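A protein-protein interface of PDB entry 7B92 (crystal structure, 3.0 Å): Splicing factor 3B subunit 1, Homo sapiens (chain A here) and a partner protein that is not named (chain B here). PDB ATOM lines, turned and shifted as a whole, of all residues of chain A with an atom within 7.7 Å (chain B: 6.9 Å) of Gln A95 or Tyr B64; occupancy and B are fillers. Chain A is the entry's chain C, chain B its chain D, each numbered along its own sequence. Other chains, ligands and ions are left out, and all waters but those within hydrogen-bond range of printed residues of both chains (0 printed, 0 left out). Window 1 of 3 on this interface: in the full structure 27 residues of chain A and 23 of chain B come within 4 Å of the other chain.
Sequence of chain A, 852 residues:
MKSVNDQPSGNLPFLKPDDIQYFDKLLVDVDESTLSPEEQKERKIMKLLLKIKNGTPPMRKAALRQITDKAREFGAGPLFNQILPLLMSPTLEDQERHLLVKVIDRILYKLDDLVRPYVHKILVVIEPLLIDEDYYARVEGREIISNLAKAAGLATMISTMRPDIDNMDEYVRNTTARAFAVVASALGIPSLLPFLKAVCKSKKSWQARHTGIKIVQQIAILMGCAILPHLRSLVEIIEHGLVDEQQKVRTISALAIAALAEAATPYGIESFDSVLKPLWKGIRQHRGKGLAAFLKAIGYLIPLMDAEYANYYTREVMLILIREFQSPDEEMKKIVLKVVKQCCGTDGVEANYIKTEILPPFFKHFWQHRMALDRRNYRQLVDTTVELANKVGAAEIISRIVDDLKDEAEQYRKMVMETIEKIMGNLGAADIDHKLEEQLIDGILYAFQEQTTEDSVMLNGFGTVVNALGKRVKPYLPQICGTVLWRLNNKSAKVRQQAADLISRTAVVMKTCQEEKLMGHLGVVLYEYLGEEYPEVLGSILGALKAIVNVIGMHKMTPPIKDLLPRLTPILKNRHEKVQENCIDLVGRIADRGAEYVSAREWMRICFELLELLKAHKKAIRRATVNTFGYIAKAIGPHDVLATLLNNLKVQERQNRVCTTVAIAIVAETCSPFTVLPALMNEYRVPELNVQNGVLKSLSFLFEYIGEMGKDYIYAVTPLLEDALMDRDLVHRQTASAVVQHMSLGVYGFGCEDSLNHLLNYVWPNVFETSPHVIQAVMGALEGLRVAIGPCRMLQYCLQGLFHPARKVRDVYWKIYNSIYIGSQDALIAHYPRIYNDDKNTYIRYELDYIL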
ATOM      1  N   ILE A  52      12.868  15.894  -3.468  1.00  0.00           N
ATOM      2  CA  ILE A  52      12.605  17.077  -2.648  1.00  0.00           C
ATOM      3  C   ILE A  52      13.746  18.082  -2.767  1.00  0.00           C
ATOM      4  O   ILE A  52      13.528  19.261  -3.070  1.00  0.00           O
ATOM      5  CB  ILE A  52      12.370  16.680  -1.179  1.00  0.00           C
ATOM      6  CG1 ILE A  52      11.018  15.986  -1.010  1.00  0.00           C
ATOM      7  CG2 ILE A  52      12.461  17.903  -0.277  1.00  0.00           C
ATOM      8  CD1 ILE A  52      10.709  15.588   0.418  1.00  0.00           C
ATOM      9  N   LYS A  53      14.977  17.632  -2.522  1.00  0.00           N
ATOM     10  CA  LYS A  53      16.118  18.541  -2.445  1.00  0.00           C
ATOM     11  C   LYS A  53      16.398  19.200  -3.790  1.00  0.00           C
ATOM     12  O   LYS A  53      16.364  20.429  -3.911  1.00  0.00           O
ATOM     13  CB  LYS A  53      17.345  17.780  -1.939  1.00  0.00           C
ATOM     14  CG  LYS A  53      18.608  18.609  -1.837  1.00  0.00           C
ATOM     15  CD  LYS A  53      19.734  17.786  -1.235  1.00  0.00           C
ATOM     16  CE  LYS A  53      21.071  18.492  -1.364  1.00  0.00           C
ATOM     17  NZ  LYS A  53      21.451  18.697  -2.789  1.00  0.00           N
ATOM     18  N   ARG A  60       8.820  19.064  -6.193  1.00  0.00           N
ATOM     19  CA  ARG A  60       8.977  19.263  -4.756  1.00  0.00           C
ATOM     20  C   ARG A  60       7.647  19.105  -4.028  1.00  0.00           C
ATOM     21  O   ARG A  60       7.570  18.426  -2.998  1.00  0.00           O
ATOM     22  CB  ARG A  60       9.586  20.637  -4.478  1.00  0.00           C
ATOM     23  CG  ARG A  60      11.041  20.773  -4.907  1.00  0.00           C
ATOM     24  CD  ARG A  60      11.623  22.108  -4.471  1.00  0.00           C
ATOM     25  NE  ARG A  60      11.032  23.234  -5.189  1.00  0.00           N
ATOM     26  CZ  ARG A  60      10.970  24.473  -4.713  1.00  0.00           C
ATOM     27  NH1 ARG A  60      11.449  24.748  -3.509  1.00  0.00           N
ATOM     28  NH2 ARG A  60      10.418  25.438  -5.436  1.00  0.00           N
ATOM     29  N   LEU A  92      25.843  21.923   2.335  1.00  0.00           N
ATOM     30  CA  LEU A  92      24.393  22.032   2.249  1.00  0.00           C
ATOM     31  C   LEU A  92      24.007  23.500   2.099  1.00  0.00           C
ATOM     32  O   LEU A  92      24.320  24.320   2.968  1.00  0.00           O
ATOM     33  CB  LEU A  92      23.727  21.422   3.482  1.00  0.00           C
ATOM     34  CG  LEU A  92      22.202  21.278   3.426  1.00  0.00           C
ATOM     35  CD1 LEU A  92      21.787  20.247   2.388  1.00  0.00           C
ATOM     36  CD2 LEU A  92      21.633  20.927   4.794  1.00  0.00           C
ATOM     37  N   GLU A  93      23.336  23.823   0.995  1.00  0.00           N
ATOM     38  CA  GLU A  93      22.843  25.177   0.782  1.00  0.00           C
ATOM     39  C   GLU A  93      21.809  25.536   1.844  1.00  0.00           C
ATOM     40  O   GLU A  93      21.137  24.667   2.406  1.00  0.00           O
ATOM     41  CB  GLU A  93      22.228  25.308  -0.612  1.00  0.00           C
ATOM     42  CG  GLU A  93      23.140  24.878  -1.753  1.00  0.00           C
ATOM     43  CD  GLU A  93      24.155  25.938  -2.133  1.00  0.00           C
ATOM     44  OE1 GLU A  93      24.061  27.073  -1.620  1.00  0.00           O
ATOM     45  OE2 GLU A  93      25.048  25.636  -2.954  1.00  0.00           O
ATOM     46  N   ASP A  94      21.683  26.839   2.119  1.00  0.00           N
ATOM     47  CA  ASP A  94      20.735  27.288   3.136  1.00  0.00           C
ATOM     48  C   ASP A  94      19.297  26.981   2.731  1.00  0.00           C
ATOM     49  O   ASP A  94      18.461  26.644   3.580  1.00  0.00           O
ATOM     50  CB  ASP A  94      20.912  28.783   3.403  1.00  0.00           C
ATOM     51  CG  ASP A  94      22.268  29.116   3.998  1.00  0.00           C
ATOM     52  OD1 ASP A  94      22.860  28.240   4.662  1.00  0.00           O
ATOM     53  OD2 ASP A  94      22.738  30.259   3.814  1.00  0.00           O
ATOM     54  N   GLN A  95      18.990  27.080   1.436  1.00  0.00           N
ATOM     55  CA  GLN A  95      17.638  26.782   0.979  1.00  0.00           C
ATOM     56  C   GLN A  95      17.356  25.286   1.027  1.00  0.00           C
ATOM     57  O   GLN A  95      16.229  24.869   1.323  1.00  0.00           O
ATOM     58  CB  GLN A  95      17.430  27.334  -0.429  1.00  0.00           C
ATOM     59  CG  GLN A  95      17.541  28.848  -0.506  1.00  0.00           C
ATOM     60  CD  GLN A  95      16.586  29.556   0.443  1.00  0.00           C
ATOM     61  OE1 GLN A  95      15.455  29.114   0.652  1.00  0.00           O
ATOM     62  NE2 GLN A  95      17.043  30.658   1.027  1.00  0.00           N
ATOM     63  N   GLU A  96      18.366  24.461   0.744  1.00  0.00           N
ATOM     64  CA  GLU A  96      18.213  23.025   0.945  1.00  0.00           C
ATOM     65  C   GLU A  96      17.965  22.708   2.415  1.00  0.00           C
ATOM     66  O   GLU A  96      17.134  21.851   2.744  1.00  0.00           O
ATOM     67  CB  GLU A  96      19.451  22.291   0.430  1.00  0.00           C
ATOM     68  CG  GLU A  96      19.711  22.487  -1.056  1.00  0.00           C
ATOM     69  CD  GLU A  96      21.056  21.941  -1.498  1.00  0.00           C
ATOM     70  OE1 GLU A  96      21.944  21.765  -0.636  1.00  0.00           O
ATOM     71  OE2 GLU A  96      21.226  21.680  -2.709  1.00  0.00           O
ATOM     72  N   ARG A  97      18.669  23.399   3.317  1.00  0.00           N
ATOM     73  CA  ARG A  97      18.417  23.211   4.741  1.00  0.00           C
ATOM     74  C   ARG A  97      16.996  23.621   5.102  1.00  0.00           C
ATOM     75  O   ARG A  97      16.351  22.977   5.936  1.00  0.00           O
ATOM     76  CB  ARG A  97      19.433  23.997   5.572  1.00  0.00           C
ATOM     77  CG  ARG A  97      19.276  23.794   7.074  1.00  0.00           C
ATOM     78  CD  ARG A  97      20.363  24.499   7.874  1.00  0.00           C
ATOM     79  NE  ARG A  97      20.239  25.951   7.813  1.00  0.00           N
ATOM     80  CZ  ARG A  97      21.062  26.741   7.133  1.00  0.00           C
ATOM     81  NH1 ARG A  97      22.077  26.217   6.460  1.00  0.00           N
ATOM     82  NH2 ARG A  97      20.872  28.054   7.128  1.00  0.00           N
ATOM     83  N   HIS A  98      16.481  24.678   4.470  1.00  0.00           N
ATOM     84  CA  HIS A  98      15.115  25.102   4.765  1.00  0.00           C
ATOM     85  C   HIS A  98      14.095  24.088   4.252  1.00  0.00           C
ATOM     86  O   HIS A  98      13.084  23.822   4.916  1.00  0.00           O
ATOM     87  CB  HIS A  98      14.850  26.482   4.167  1.00  0.00           C
ATOM     88  CG  HIS A  98      13.543  27.076   4.589  1.00  0.00           C
ATOM     89  ND1 HIS A  98      12.586  27.490   3.688  1.00  0.00           N
ATOM     90  CD2 HIS A  98      13.031  27.315   5.819  1.00  0.00           C
ATOM     91  CE1 HIS A  98      11.543  27.964   4.344  1.00  0.00           C
ATOM     92  NE2 HIS A  98      11.788  27.872   5.639  1.00  0.00           N
ATOM     93  N   LEU A  99      14.342  23.513   3.073  1.00  0.00           N
ATOM     94  CA  LEU A  99      13.461  22.463   2.566  1.00  0.00           C
ATOM     95  C   LEU A  99      13.474  21.245   3.482  1.00  0.00           C
ATOM     96  O   LEU A  99      12.427  20.637   3.741  1.00  0.00           O
ATOM     97  CB  LEU A  99      13.869  22.066   1.148  1.00  0.00           C
ATOM     98  CG  LEU A  99      13.135  22.747  -0.009  1.00  0.00           C
ATOM     99  CD1 LEU A  99      13.335  24.256   0.017  1.00  0.00           C
ATOM    100  CD2 LEU A  99      13.585  22.166  -1.337  1.00  0.00           C
ATOM    101  N   LEU A 100      14.656  20.870   3.978  1.00  0.00           N
ATOM    102  CA  LEU A 100      14.731  19.766   4.929  1.00  0.00           C
ATOM    103  C   LEU A 100      13.990  20.103   6.217  1.00  0.00           C
ATOM    104  O   LEU A 100      13.326  19.242   6.801  1.00  0.00           O
ATOM    105  CB  LEU A 100      16.189  19.411   5.216  1.00  0.00           C
ATOM    106  CG  LEU A 100      16.788  18.266   4.395  1.00  0.00           C
ATOM    107  CD1 LEU A 100      16.646  18.515   2.904  1.00  0.00           C
ATOM    108  CD2 LEU A 100      18.247  18.058   4.756  1.00  0.00           C
ATOM    109  N   VAL A 101      14.084  21.353   6.670  1.00  0.00           N
ATOM    110  CA  VAL A 101      13.351  21.768   7.861  1.00  0.00           C
ATOM    111  C   VAL A 101      11.851  21.613   7.644  1.00  0.00           C
ATOM    112  O   VAL A 101      11.122  21.129   8.522  1.00  0.00           O
ATOM    113  CB  VAL A 101      13.726  23.215   8.232  1.00  0.00           C
ATOM    114  CG1 VAL A 101      12.699  23.812   9.182  1.00  0.00           C
ATOM    115  CG2 VAL A 101      15.111  23.256   8.840  1.00  0.00           C
ATOM    116  N   LYS A 102      11.369  22.013   6.468  1.00  0.00           N
ATOM    117  CA  LYS A 102       9.939  21.918   6.193  1.00  0.00           C
ATOM    118  C   LYS A 102       9.485  20.464   6.113  1.00  0.00           C
ATOM    119  O   LYS A 102       8.426  20.107   6.646  1.00  0.00           O
ATOM    120  CB  LYS A 102       9.596  22.669   4.907  1.00  0.00           C
ATOM    121  CG  LYS A 102       9.720  24.184   5.035  1.00  0.00           C
ATOM    122  CD  LYS A 102       8.962  24.698   6.257  1.00  0.00           C
ATOM    123  CE  LYS A 102       9.066  26.212   6.388  1.00  0.00           C
ATOM    124  NZ  LYS A 102       8.347  26.737   7.585  1.00  0.00           N
ATOM    125  N   TYR A 136      19.032  32.683  10.131  1.00  0.00           N
ATOM    126  CA  TYR A 136      18.015  31.766   9.630  1.00  0.00           C
ATOM    127  C   TYR A 136      18.312  30.327  10.022  1.00  0.00           C
ATOM    128  O   TYR A 136      17.385  29.521  10.149  1.00  0.00           O
ATOM    129  CB  TYR A 136      17.881  31.912   8.115  1.00  0.00           C
ATOM    130  CG  TYR A 136      17.310  33.252   7.709  1.00  0.00           C
ATOM    131  CD1 TYR A 136      15.940  33.480   7.737  1.00  0.00           C
ATOM    132  CD2 TYR A 136      18.138  34.295   7.313  1.00  0.00           C
ATOM    133  CE1 TYR A 136      15.410  34.704   7.378  1.00  0.00           C
ATOM    134  CE2 TYR A 136      17.616  35.522   6.949  1.00  0.00           C
ATOM    135  CZ  TYR A 136      16.251  35.721   6.983  1.00  0.00           C
ATOM    136  OH  TYR A 136      15.724  36.940   6.623  1.00  0.00           O
ATOM    137  N   GLU A 140      15.584  28.080  11.887  1.00  0.00           N
ATOM    138  CA  GLU A 140      15.229  26.730  11.462  1.00  0.00           C
ATOM    139  C   GLU A 140      15.395  25.727  12.599  1.00  0.00           C
ATOM    140  O   GLU A 140      14.546  24.843  12.787  1.00  0.00           O
ATOM    141  CB  GLU A 140      16.082  26.326  10.260  1.00  0.00           C
ATOM    142  CG  GLU A 140      15.709  27.040   8.971  1.00  0.00           C
ATOM    143  CD  GLU A 140      16.836  27.041   7.961  1.00  0.00           C
ATOM    144  OE1 GLU A 140      17.965  26.656   8.333  1.00  0.00           O
ATOM    145  OE2 GLU A 140      16.598  27.428   6.798  1.00  0.00           O
ATOM    146  N   ILE B  55       4.359  40.610  -0.585  1.00  0.00           N
ATOM    147  CA  ILE B  55       4.696  39.252  -0.990  1.00  0.00           C
ATOM    148  C   ILE B  55       4.512  38.314   0.197  1.00  0.00           C
ATOM    149  O   ILE B  55       4.514  38.730   1.358  1.00  0.00           O
ATOM    150  CB  ILE B  55       6.136  39.137  -1.542  1.00  0.00           C
ATOM    151  CG1 ILE B  55       7.152  39.558  -0.485  1.00  0.00           C
ATOM    152  CG2 ILE B  55       6.302  39.979  -2.795  1.00  0.00           C
ATOM    153  CD1 ILE B  55       8.580  39.424  -0.941  1.00  0.00           C
ATOM    154  N   GLU B  58       7.106  33.010   2.333  1.00  0.00           N
ATOM    155  CA  GLU B  58       8.051  32.042   1.787  1.00  0.00           C
ATOM    156  C   GLU B  58       8.978  32.688   0.767  1.00  0.00           C
ATOM    157  O   GLU B  58      10.165  32.348   0.697  1.00  0.00           O
ATOM    158  CB  GLU B  58       7.298  30.864   1.171  1.00  0.00           C
ATOM    159  CG  GLU B  58       6.560  30.008   2.194  1.00  0.00           C
ATOM    160  CD  GLU B  58       7.491  29.357   3.211  1.00  0.00           C
ATOM    161  OE1 GLU B  58       8.651  29.054   2.855  1.00  0.00           O
ATOM    162  OE2 GLU B  58       7.061  29.154   4.368  1.00  0.00           O
ATOM    163  N   CYS B  59       8.464  33.630  -0.021  1.00  0.00           N
ATOM    164  CA  CYS B  59       9.284  34.310  -1.015  1.00  0.00           C
ATOM    165  C   CYS B  59      10.227  35.336  -0.406  1.00  0.00           C
ATOM    166  O   CYS B  59      11.109  35.838  -1.111  1.00  0.00           O
ATOM    167  CB  CYS B  59       8.389  34.983  -2.060  1.00  0.00           C
ATOM    168  SG  CYS B  59       7.446  33.830  -3.087  1.00  0.00           S
ATOM    169  N   ASN B  60      10.071  35.651   0.878  1.00  0.00           N
ATOM    170  CA  ASN B  60      10.904  36.634   1.553  1.00  0.00           C
ATOM    171  C   ASN B  60      11.872  36.002   2.545  1.00  0.00           C
ATOM    172  O   ASN B  60      12.699  36.713   3.125  1.00  0.00           O
ATOM    173  CB  ASN B  60      10.018  37.658   2.274  1.00  0.00           C
ATOM    174  CG  ASN B  60      10.757  38.932   2.617  1.00  0.00           C
ATOM    175  OD1 ASN B  60      11.579  39.416   1.839  1.00  0.00           O
ATOM    176  ND2 ASN B  60      10.475  39.479   3.794  1.00  0.00           N
ATOM    177  N   TYR B  61      11.799  34.691   2.745  1.00  0.00           N
ATOM    178  CA  TYR B  61      12.572  34.033   3.787  1.00  0.00           C
ATOM    179  C   TYR B  61      14.025  33.842   3.369  1.00  0.00           C
ATOM    180  O   TYR B  61      14.339  33.644   2.192  1.00  0.00           O
ATOM    181  CB  TYR B  61      11.953  32.676   4.130  1.00  0.00           C
ATOM    182  CG  TYR B  61      12.654  31.947   5.254  1.00  0.00           C
ATOM    183  CD1 TYR B  61      12.307  32.180   6.576  1.00  0.00           C
ATOM    184  CD2 TYR B  61      13.656  31.020   4.992  1.00  0.00           C
ATOM    185  CE1 TYR B  61      12.942  31.520   7.608  1.00  0.00           C
ATOM    186  CE2 TYR B  61      14.299  30.355   6.017  1.00  0.00           C
ATOM    187  CZ  TYR B  61      13.937  30.607   7.324  1.00  0.00           C
ATOM    188  OH  TYR B  61      14.567  29.949   8.355  1.00  0.00           O
ATOM    189  N   GLY B  62      14.914  33.910   4.357  1.00  0.00           N
ATOM    190  CA  GLY B  62      16.297  33.513   4.139  1.00  0.00           C
ATOM    191  C   GLY B  62      17.042  34.495   3.262  1.00  0.00           C
ATOM    192  O   GLY B  62      16.984  35.714   3.459  1.00  0.00           O
ATOM    193  N   SER B  63      17.763  33.957   2.276  1.00  0.00           N
ATOM    194  CA  SER B  63      18.551  34.771   1.359  1.00  0.00           C
ATOM    195  C   SER B  63      17.697  35.533   0.357  1.00  0.00           C
ATOM    196  O   SER B  63      18.253  36.283  -0.454  1.00  0.00           O
ATOM    197  CB  SER B  63      19.560  33.890   0.621  1.00  0.00           C
ATOM    198  OG  SER B  63      18.914  32.794  -0.003  1.00  0.00           O
ATOM    199  N   TYR B  64      16.377  35.361   0.387  1.00  0.00           N
ATOM    200  CA  TYR B  64      15.470  36.099  -0.479  1.00  0.00           C
ATOM    201  C   TYR B  64      14.886  37.331   0.201  1.00  0.00           C
ATOM    202  O   TYR B  64      13.987  37.967  -0.356  1.00  0.00           O
ATOM    203  CB  TYR B  64      14.347  35.186  -0.967  1.00  0.00           C
ATOM    204  CG  TYR B  64      14.843  33.993  -1.748  1.00  0.00           C
ATOM    205  CD1 TYR B  64      15.163  34.106  -3.094  1.00  0.00           C
ATOM    206  CD2 TYR B  64      14.989  32.754  -1.141  1.00  0.00           C
ATOM    207  CE1 TYR B  64      15.619  33.017  -3.813  1.00  0.00           C
ATOM    208  CE2 TYR B  64      15.442  31.660  -1.852  1.00  0.00           C
ATOM    209  CZ  TYR B  64      15.756  31.797  -3.186  1.00  0.00           C
ATOM    210  OH  TYR B  64      16.208  30.707  -3.895  1.00  0.00           O
ATOM    211  N   GLN B  65      15.367  37.674   1.394  1.00  0.00           N
ATOM    212  CA  GLN B  65      14.951  38.909   2.042  1.00  0.00           C
ATOM    213  C   GLN B  65      15.401  40.104   1.212  1.00  0.00           C
ATOM    214  O   GLN B  65      16.584  40.239   0.886  1.00  0.00           O
ATOM    215  CB  GLN B  65      15.533  38.986   3.454  1.00  0.00           C
ATOM    216  CG  GLN B  65      15.490  40.376   4.079  1.00  0.00           C
ATOM    217  CD  GLN B  65      14.078  40.909   4.246  1.00  0.00           C
ATOM    218  OE1 GLN B  65      13.194  40.217   4.756  1.00  0.00           O
ATOM    219  NE2 GLN B  65      13.861  42.146   3.815  1.00  0.00           N
ATOM    220  N   GLY B  66      14.448  40.965   0.860  1.00  0.00           N
ATOM    221  CA  GLY B  66      14.765  42.128   0.054  1.00  0.00           C
ATOM    222  C   GLY B  66      15.236  41.808  -1.343  1.00  0.00           C
ATOM    223  O   GLY B  66      15.899  42.636  -1.973  1.00  0.00           O
ATOM    224  N   ARG B  67      14.916  40.620  -1.844  1.00  0.00           N
ATOM    225  CA  ARG B  67      15.328  40.222  -3.178  1.00  0.00           C
ATOM    226  C   ARG B  67      14.352  40.770  -4.212  1.00  0.00           C
ATOM    227  O   ARG B  67      13.176  41.006  -3.921  1.00  0.00           O
ATOM    228  CB  ARG B  67      15.411  38.698  -3.269  1.00  0.00           C
ATOM    229  CG  ARG B  67      16.243  38.168  -4.422  1.00  0.00           C
ATOM    230  CD  ARG B  67      17.657  38.734  -4.413  1.00  0.00           C
ATOM    231  NE  ARG B  67      18.375  38.484  -3.167  1.00  0.00           N
ATOM    232  CZ  ARG B  67      19.660  38.772  -2.979  1.00  0.00           C
ATOM    233  NH1 ARG B  67      20.240  38.516  -1.814  1.00  0.00           N
ATOM    234  NH2 ARG B  67      20.373  39.305  -3.963  1.00  0.00           N
ATOM    235  N   CYS B  68      14.856  40.981  -5.426  1.00  0.00           N
ATOM    236  CA  CYS B  68      14.047  41.570  -6.483  1.00  0.00           C
ATOM    237  C   CYS B  68      12.910  40.633  -6.869  1.00  0.00           C
ATOM    238  O   CYS B  68      13.115  39.430  -7.058  1.00  0.00           O
ATOM    239  CB  CYS B  68      14.917  41.885  -7.699  1.00  0.00           C
ATOM    240  SG  CYS B  68      14.004  42.357  -9.184  1.00  0.00           S
ATOM    241  N   GLY B  72      15.409  38.767  -9.375  1.00  0.00           N
ATOM    242  CA  GLY B  72      15.907  38.009  -8.246  1.00  0.00           C
ATOM    243  C   GLY B  72      17.293  38.453  -7.832  1.00  0.00           C
ATOM    244  O   GLY B  72      18.110  37.640  -7.390  1.00  0.00           O
ATOM    245  N   LYS B  97       5.374  37.456  -6.975  1.00  0.00           N
ATOM    246  CA  LYS B  97       6.754  37.010  -7.119  1.00  0.00           C
ATOM    247  C   LYS B  97       6.888  36.065  -8.307  1.00  0.00           C
ATOM    248  O   LYS B  97       6.167  35.068  -8.408  1.00  0.00           O
ATOM    249  CB  LYS B  97       7.224  36.322  -5.842  1.00  0.00           C
ATOM    250  CG  LYS B  97       8.677  35.878  -5.862  1.00  0.00           C
ATOM    251  CD  LYS B  97       9.623  37.060  -5.798  1.00  0.00           C
ATOM    252  CE  LYS B  97      11.069  36.601  -5.702  1.00  0.00           C
ATOM    253  NZ  LYS B  97      11.311  35.761  -4.496  1.00  0.00           N
ATOM    254  N   SER B 104      15.356  24.826  -9.336  1.00  0.00           N
ATOM    255  CA  SER B 104      15.210  24.533  -7.923  1.00  0.00           C
ATOM    256  C   SER B 104      15.600  25.762  -7.098  1.00  0.00           C
ATOM    257  O   SER B 104      15.589  26.894  -7.604  1.00  0.00           O
ATOM    258  CB  SER B 104      16.046  23.299  -7.575  1.00  0.00           C
ATOM    259  OG  SER B 104      15.891  22.956  -6.209  1.00  0.00           O
ATOM    260  N   LYS B 105      15.944  25.539  -5.830  1.00  0.00           N
ATOM    261  CA  LYS B 105      16.330  26.620  -4.932  1.00  0.00           C
ATOM    262  C   LYS B 105      17.824  26.914  -4.954  1.00  0.00           C
ATOM    263  O   LYS B 105      18.253  27.902  -4.347  1.00  0.00           O
ATOM    264  CB  LYS B 105      15.899  26.299  -3.497  1.00  0.00           C
ATOM    265  CG  LYS B 105      14.408  26.072  -3.330  1.00  0.00           C
ATOM    266  CD  LYS B 105      13.611  27.273  -3.822  1.00  0.00           C
ATOM    267  CE  LYS B 105      13.878  28.513  -2.982  1.00  0.00           C
ATOM    268  NZ  LYS B 105      13.193  29.713  -3.541  1.00  0.00           N
ATOM    269  N   THR B 106      18.621  26.093  -5.635  1.00  0.00           N
ATOM    270  CA  THR B 106      20.061  26.296  -5.691  1.00  0.00           C
ATOM    271  C   THR B 106      20.536  26.869  -7.018  1.00  0.00           C
ATOM    272  O   THR B 106      21.669  27.358  -7.092  1.00  0.00           O
ATOM    273  CB  THR B 106      20.791  24.976  -5.428  1.00  0.00           C
ATOM    274  OG1 THR B 106      20.433  24.020  -6.436  1.00  0.00           O
ATOM    275  CG2 THR B 106      20.407  24.432  -4.066  1.00  0.00           C
ATOM    276  N   ASP B 107      19.707  26.820  -8.057  1.00  0.00           N
ATOM    277  CA  ASP B 107      20.105  27.333  -9.360  1.00  0.00           C
ATOM    278  C   ASP B 107      20.181  28.854  -9.322  1.00  0.00           C
ATOM    279  O   ASP B 107      19.231  29.522  -8.901  1.00  0.00           O
ATOM    280  CB  ASP B 107      19.118  26.872 -10.433  1.00  0.00           C
ATOM    281  CG  ASP B 107      18.973  25.361 -10.479  1.00  0.00           C
ATOM    282  OD1 ASP B 107      19.901  24.660 -10.022  1.00  0.00           O
ATOM    283  OD2 ASP B 107      17.935  24.872 -10.973  1.00  0.00           O
ATOM    284  N   LEU B 108      21.319  29.394  -9.758  1.00  0.00           N
ATOM    285  CA  LEU B 108      21.573  30.835  -9.760  1.00  0.00           C
ATOM    286  C   LEU B 108      21.408  31.444  -8.365  1.00  0.00           C
ATOM    287  O   LEU B 108      20.340  31.943  -8.010  1.00  0.00           O
ATOM    288  CB  LEU B 108      20.654  31.543 -10.762  1.00  0.00           C
ATOM    289  CG  LEU B 108      20.906  33.036 -10.993  1.00  0.00           C
ATOM    290  CD1 LEU B 108      22.322  33.278 -11.493  1.00  0.00           C
ATOM    291  CD2 LEU B 108      19.884  33.606 -11.966  1.00  0.00           C
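Of chain B, only Ser B63 (3.0 Å), Tyr B64 (3.3 Å) and Lys B105 (3.6 Å) come within 4 Å of Gln A95. Printed residues of chain B within 4 Å of Tyr A136: Tyr B61 (3.4 Å), Gly B62 (3.2 Å) and Gln B65 (3.8 Å). Ser B63 touches one residue of chain A. Of the printed residues of chain A, Ser B104 touches Lys A53. Printed residues of chain A within 4 Å of Lys B105: Arg A60 (3.2 Å), Gln A95 (3.6 Å) and Leu A99 (3.96 Å). The nearest printed residue of chain B that does not touch Tyr A136 is Asn B60 (4.6 Å).
Of the 19 printed residues of chain B, 9 touch a printed residue of chain A. Printed residues of chain B that touch a printed residue of chain A: Glu B58, Tyr B61, Gly B62, Ser B63, Tyr B64, Gln B65, Ser B104, Lys B105 and Thr B106. Hydrophobic or aromatic side chains of chain B that line the printed part of chain A: Tyr B61 and Tyr B64. Among the printed residues, 14 pairs touch across the chains. Among the printed residues, no Asp or Glu carboxylate lies within 4 Å of a Lys or Arg side-chain nitrogen of the other chain.
Among the printed residues, pairs that only touch across the chains: Arg A60 with Lys B105, Glu A93 with Thr B106, Gln A95 with Tyr B64, Gln A95 with Lys B105, Glu A96 with Thr B106, His A98 with Glu B58, His A98 with Tyr B61, Leu A99 with Lys B105, Tyr A136 with Gly B62, Tyr A136 with Gln B65 and Glu A140 with Tyr B61.
OG of Ser B104 sits at hydrogen-bond distance from O of Lys A53, at 3.4 Å. NE2 of Gln A95 lies within hydrogen-bond range of OG of Ser B63, 3.0 Å away. The backbone carbonyl oxygen (O) of Tyr A136 sits at hydrogen-bond distance from the side-chain hydroxyl (OH) of Tyr B61, at 3.4 Å.
OE2 of Glu A96 lies within salt-bridge range of NZ of Lys A53, at 3.0 Å. The guanidinium group (NE) of Arg A97 is in salt-bridge range of the side-chain carboxylate (OE1) of Glu A140, 2.4 Å away. OE1 of Gln B65 is in hydrogen-bond range of ND2 of Asn B60 (3.0 Å). O of Ser B63 is in hydrogen-bond range of NH1 of Arg B67, 3.3 Å away. The side-chain amino group (NZ) of Lys B105 sits at hydrogen-bond distance from the side-chain hydroxyl (OH) of Tyr B64 (3.2 Å). The backbone NH (N) of Ser B104 sits at hydrogen-bond distance from the side-chain carboxylate (OD2) of Asp B107 (3.1 Å).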
